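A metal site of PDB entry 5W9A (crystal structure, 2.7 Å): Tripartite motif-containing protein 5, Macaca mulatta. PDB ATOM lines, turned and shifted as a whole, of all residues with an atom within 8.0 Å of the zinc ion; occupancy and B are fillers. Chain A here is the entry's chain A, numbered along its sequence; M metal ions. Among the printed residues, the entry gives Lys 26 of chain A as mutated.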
ATOM      1  N   HIS A   2      -4.159 -14.354   9.554  1.00  0.00           N
ATOM      2  CA  HIS A   2      -4.538 -14.397  10.954  1.00  0.00           C
ATOM      3  C   HIS A   2      -3.493 -15.145  11.780  1.00  0.00           C
ATOM      4  O   HIS A   2      -2.653 -15.875  11.247  1.00  0.00           O
ATOM      5  CB  HIS A   2      -5.913 -15.039  11.123  1.00  0.00           C
ATOM      6  CG  HIS A   2      -7.032 -14.208  10.596  1.00  0.00           C
ATOM      7  ND1 HIS A   2      -8.352 -14.607  10.654  1.00  0.00           N
ATOM      8  CD2 HIS A   2      -7.035 -12.997   9.999  1.00  0.00           C
ATOM      9  CE1 HIS A   2      -9.115 -13.676  10.107  1.00  0.00           C
ATOM     10  NE2 HIS A   2      -8.347 -12.692   9.704  1.00  0.00           N
ATOM     11  N   CYS A   3      -3.562 -14.957  13.093  1.00  0.00           N
ATOM     12  CA  CYS A   3      -2.565 -15.503  13.999  1.00  0.00           C
ATOM     13  C   CYS A   3      -2.756 -17.010  14.174  1.00  0.00           C
ATOM     14  O   CYS A   3      -3.883 -17.506  14.172  1.00  0.00           O
ATOM     15  CB  CYS A   3      -2.635 -14.812  15.361  1.00  0.00           C
ATOM     16  SG  CYS A   3      -1.391 -15.369  16.549  1.00  0.00           S
ATOM     17  N   ALA A   4      -1.642 -17.720  14.320  1.00  0.00           N
ATOM     18  CA  ALA A   4      -1.695 -19.162  14.526  1.00  0.00           C
ATOM     19  C   ALA A   4      -2.001 -19.527  15.977  1.00  0.00           C
ATOM     20  O   ALA A   4      -2.625 -20.570  16.225  1.00  0.00           O
ATOM     21  CB  ALA A   4      -0.382 -19.811  14.088  1.00  0.00           C
ATOM     22  N   ARG A   5      -1.575 -18.705  16.933  1.00  0.00           N
ATOM     23  CA  ARG A   5      -1.776 -19.045  18.336  1.00  0.00           C
ATOM     24  C   ARG A   5      -3.185 -18.711  18.805  1.00  0.00           C
ATOM     25  O   ARG A   5      -3.797 -19.485  19.547  1.00  0.00           O
ATOM     26  CB  ARG A   5      -0.744 -18.322  19.211  1.00  0.00           C
ATOM     27  CG  ARG A   5      -0.839 -18.690  20.685  1.00  0.00           C
ATOM     28  CD  ARG A   5       0.144 -17.899  21.547  1.00  0.00           C
ATOM     29  NE  ARG A   5       1.531 -18.182  21.208  1.00  0.00           N
ATOM     30  CZ  ARG A   5       2.308 -17.372  20.505  1.00  0.00           C
ATOM     31  NH1 ARG A   5       1.834 -16.221  20.047  1.00  0.00           N
ATOM     32  NH2 ARG A   5       3.568 -17.705  20.256  1.00  0.00           N
ATOM     33  N   HIS A   6      -3.722 -17.565  18.390  1.00  0.00           N
ATOM     34  CA  HIS A   6      -5.026 -17.097  18.837  1.00  0.00           C
ATOM     35  C   HIS A   6      -6.076 -17.052  17.741  1.00  0.00           C
ATOM     36  O   HIS A   6      -7.240 -17.385  17.996  1.00  0.00           O
ATOM     37  CB  HIS A   6      -4.905 -15.713  19.477  1.00  0.00           C
ATOM     38  CG  HIS A   6      -4.111 -15.701  20.741  1.00  0.00           C
ATOM     39  ND1 HIS A   6      -2.750 -15.460  20.778  1.00  0.00           N
ATOM     40  CD2 HIS A   6      -4.480 -15.903  22.037  1.00  0.00           C
ATOM     41  CE1 HIS A   6      -2.323 -15.512  22.028  1.00  0.00           C
ATOM     42  NE2 HIS A   6      -3.356 -15.780  22.800  1.00  0.00           N
ATOM     43  N   GLY A   7      -5.714 -16.644  16.527  1.00  0.00           N
ATOM     44  CA  GLY A   7      -6.651 -16.574  15.422  1.00  0.00           C
ATOM     45  C   GLY A   7      -7.007 -15.177  14.977  1.00  0.00           C
ATOM     46  O   GLY A   7      -7.769 -15.032  14.011  1.00  0.00           O
ATOM     47  N   GLU A   8      -6.508 -14.138  15.647  1.00  0.00           N
ATOM     48  CA  GLU A   8      -6.795 -12.764  15.274  1.00  0.00           C
ATOM     49  C   GLU A   8      -5.770 -12.261  14.254  1.00  0.00           C
ATOM     50  O   GLU A   8      -4.748 -12.900  13.987  1.00  0.00           O
ATOM     51  CB  GLU A   8      -6.811 -11.872  16.514  1.00  0.00           C
ATOM     52  CG  GLU A   8      -7.920 -12.190  17.492  1.00  0.00           C
ATOM     53  CD  GLU A   8      -9.279 -11.716  17.017  1.00  0.00           C
ATOM     54  OE1 GLU A   8      -9.326 -10.835  16.133  1.00  0.00           O
ATOM     55  OE2 GLU A   8     -10.299 -12.212  17.537  1.00  0.00           O
ATOM     56  N   LYS A   9      -6.064 -11.101  13.669  1.00  0.00           N
ATOM     57  CA  LYS A   9      -5.175 -10.513  12.681  1.00  0.00           C
ATOM     58  C   LYS A   9      -3.850 -10.096  13.316  1.00  0.00           C
ATOM     59  O   LYS A   9      -3.783  -9.765  14.494  1.00  0.00           O
ATOM     60  CB  LYS A   9      -5.834  -9.302  12.026  1.00  0.00           C
ATOM     61  CG  LYS A   9      -7.184  -9.593  11.383  1.00  0.00           C
ATOM     62  CD  LYS A   9      -7.804  -8.313  10.841  1.00  0.00           C
ATOM     63  CE  LYS A   9      -9.184  -8.573  10.259  1.00  0.00           C
ATOM     64  NZ  LYS A   9      -9.819  -7.323   9.761  1.00  0.00           N
ATOM     65  N   LEU A  10      -2.796 -10.121  12.497  1.00  0.00           N
ATOM     66  CA  LEU A  10      -1.476  -9.646  12.914  1.00  0.00           C
ATOM     67  C   LEU A  10      -1.321  -8.220  12.396  1.00  0.00           C
ATOM     68  O   LEU A  10      -0.799  -7.983  11.311  1.00  0.00           O
ATOM     69  CB  LEU A  10      -0.364 -10.552  12.398  1.00  0.00           C
ATOM     70  CG  LEU A  10      -0.358 -12.003  12.866  1.00  0.00           C
ATOM     71  CD1 LEU A  10      -1.071 -12.877  11.851  1.00  0.00           C
ATOM     72  CD2 LEU A  10       1.060 -12.501  13.083  1.00  0.00           C
ATOM     73  N   VAL A  20       5.456  -9.645  14.724  1.00  0.00           N
ATOM     74  CA  VAL A  20       4.073  -9.199  14.552  1.00  0.00           C
ATOM     75  C   VAL A  20       3.149 -10.168  15.269  1.00  0.00           C
ATOM     76  O   VAL A  20       3.321 -11.395  15.198  1.00  0.00           O
ATOM     77  CB  VAL A  20       3.718  -9.072  13.053  1.00  0.00           C
ATOM     78  CG1 VAL A  20       4.518  -7.952  12.416  1.00  0.00           C
ATOM     79  CG2 VAL A  20       3.952 -10.382  12.327  1.00  0.00           C
ATOM     80  N   ILE A  21       2.169  -9.623  15.996  1.00  0.00           N
ATOM     81  CA  ILE A  21       1.272 -10.438  16.815  1.00  0.00           C
ATOM     82  C   ILE A  21      -0.137  -9.872  16.717  1.00  0.00           C
ATOM     83  O   ILE A  21      -0.406  -8.977  15.914  1.00  0.00           O
ATOM     84  CB  ILE A  21       1.745 -10.478  18.276  1.00  0.00           C
ATOM     85  CG1 ILE A  21       2.021  -9.063  18.791  1.00  0.00           C
ATOM     86  CG2 ILE A  21       2.971 -11.371  18.434  1.00  0.00           C
ATOM     87  CD1 ILE A  21       2.437  -9.008  20.240  1.00  0.00           C
ATOM     88  N   CYS A  22      -1.037 -10.393  17.545  1.00  0.00           N
ATOM     89  CA  CYS A  22      -2.402  -9.896  17.649  1.00  0.00           C
ATOM     90  C   CYS A  22      -2.579  -9.211  19.004  1.00  0.00           C
ATOM     91  O   CYS A  22      -1.650  -9.114  19.807  1.00  0.00           O
ATOM     92  CB  CYS A  22      -3.419 -11.024  17.466  1.00  0.00           C
ATOM     93  SG  CYS A  22      -3.553 -12.141  18.877  1.00  0.00           S
ATOM     94  N   TRP A  23      -3.801  -8.735  19.251  1.00  0.00           N
ATOM     95  CA  TRP A  23      -4.077  -8.049  20.508  1.00  0.00           C
ATOM     96  C   TRP A  23      -4.132  -9.023  21.679  1.00  0.00           C
ATOM     97  O   TRP A  23      -3.845  -8.628  22.817  1.00  0.00           O
ATOM     98  CB  TRP A  23      -5.378  -7.246  20.402  1.00  0.00           C
ATOM     99  CG  TRP A  23      -6.579  -8.088  20.125  1.00  0.00           C
ATOM    100  CD1 TRP A  23      -6.958  -8.614  18.922  1.00  0.00           C
ATOM    101  CD2 TRP A  23      -7.588  -8.487  21.073  1.00  0.00           C
ATOM    102  NE1 TRP A  23      -8.126  -9.330  19.068  1.00  0.00           N
ATOM    103  CE2 TRP A  23      -8.528  -9.263  20.373  1.00  0.00           C
ATOM    104  CE3 TRP A  23      -7.770  -8.275  22.441  1.00  0.00           C
ATOM    105  CZ2 TRP A  23      -9.652  -9.824  20.994  1.00  0.00           C
ATOM    106  CZ3 TRP A  23      -8.881  -8.824  23.049  1.00  0.00           C
ATOM    107  CH2 TRP A  23      -9.801  -9.586  22.329  1.00  0.00           C
ATOM    108  N   LEU A  24      -4.504 -10.278  21.431  1.00  0.00           N
ATOM    109  CA  LEU A  24      -4.511 -11.268  22.496  1.00  0.00           C
ATOM    110  C   LEU A  24      -3.087 -11.612  22.947  1.00  0.00           C
ATOM    111  O   LEU A  24      -2.875 -11.911  24.135  1.00  0.00           O
ATOM    112  CB  LEU A  24      -5.242 -12.526  22.049  1.00  0.00           C
ATOM    113  CG  LEU A  24      -6.762 -12.423  21.925  1.00  0.00           C
ATOM    114  CD1 LEU A  24      -7.357 -13.709  21.364  1.00  0.00           C
ATOM    115  CD2 LEU A  24      -7.379 -12.095  23.280  1.00  0.00           C
ATOM    116  N   CYS A  25      -2.127 -11.590  22.033  1.00  0.00           N
ATOM    117  CA  CYS A  25      -0.739 -11.836  22.401  1.00  0.00           C
ATOM    118  C   CYS A  25      -0.138 -10.691  23.220  1.00  0.00           C
ATOM    119  O   CYS A  25       0.844 -10.904  23.933  1.00  0.00           O
ATOM    120  CB  CYS A  25       0.116 -12.061  21.146  1.00  0.00           C
ATOM    121  SG  CYS A  25      -0.391 -13.482  20.139  1.00  0.00           S
ATOM    122  N   LYS A  26      -0.706  -9.487  23.113  1.00  0.00           N
ATOM    123  CA  LYS A  26      -0.153  -8.350  23.852  1.00  0.00           C
ATOM    124  C   LYS A  26      -0.446  -8.435  25.344  1.00  0.00           C
ATOM    125  O   LYS A  26       0.374  -8.010  26.159  1.00  0.00           O
ATOM    126  CB  LYS A  26      -0.710  -7.044  23.272  1.00  0.00           C
ATOM    127  CG  LYS A  26      -0.075  -5.792  23.862  1.00  0.00           C
ATOM    128  CD  LYS A  26      -0.622  -4.530  23.217  1.00  0.00           C
ATOM    129  CE  LYS A  26      -2.102  -4.349  23.509  1.00  0.00           C
ATOM    130  NZ  LYS A  26      -2.634  -3.088  22.945  1.00  0.00           N
ATOM    131  N   SER A  28      -1.089 -11.347  27.061  1.00  0.00           N
ATOM    132  CA  SER A  28      -0.581 -12.559  27.670  1.00  0.00           C
ATOM    133  C   SER A  28       0.826 -12.335  28.224  1.00  0.00           C
ATOM    134  O   SER A  28       1.462 -11.310  27.978  1.00  0.00           O
ATOM    135  CB  SER A  28      -0.587 -13.709  26.653  1.00  0.00           C
ATOM    136  OG  SER A  28       0.319 -13.449  25.596  1.00  0.00           O
ATOM    137  N   HIS A  31       4.176 -11.572  25.692  1.00  0.00           N
ATOM    138  CA  HIS A  31       4.593 -10.230  25.304  1.00  0.00           C
ATOM    139  C   HIS A  31       4.162  -9.188  26.335  1.00  0.00           C
ATOM    140  O   HIS A  31       3.880  -8.043  25.994  1.00  0.00           O
ATOM    141  CB  HIS A  31       4.057  -9.846  23.923  1.00  0.00           C
ATOM    142  CG  HIS A  31       4.384 -10.825  22.843  1.00  0.00           C
ATOM    143  ND1 HIS A  31       5.625 -10.873  22.243  1.00  0.00           N
ATOM    144  CD2 HIS A  31       3.633 -11.753  22.212  1.00  0.00           C
ATOM    145  CE1 HIS A  31       5.629 -11.812  21.308  1.00  0.00           C
ATOM    146  NE2 HIS A  31       4.430 -12.355  21.274  1.00  0.00           N
HETATM  147 ZN    ZN M   1      -1.981 -13.803  18.282  1.00  0.00          ZN
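The zinc ion is bound by SG of Cys 22.
The zinc ion is bound by SG of Cys 3 (2.4 Å).
The zinc ion is bound by the side-chain sulfur (SG) of Cys 25, 2.5 Å away.
The zinc ion has three donor atoms within binding distance.
The backbone NH (N) of Leu 24 sits close to the side-chain sulfur (SG) of Cys 22 (3.3 Å).
The side-chain sulfur (SG) of Cys 3 lies close to the backbone NH (N) of His 6 (3.7 Å).
The backbone NH (N) of Arg 5 sits close to the side-chain sulfur (SG) of Cys 3, at 3.4 Å.
The backbone NH (N) of Cys 3 lies within hydrogen-bond range of the backbone carbonyl oxygen (O) of Glu 8, at 2.5 Å.
A ring nitrogen (ND1) of His 6 sits close to the side-chain sulfur of Cys 25 (3.1 Å).
SG of Cys 25 lies close to NH1 of Arg 5.
O of Cys 25 is in hydrogen-bond range of OG of Ser 28 (3.1 Å).
Merely in contact with the zinc ion: His 6 (3.1 Å).
Within 4 Å of the zinc ion: Cys 3, His 6, Cys 22 and Cys 25.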
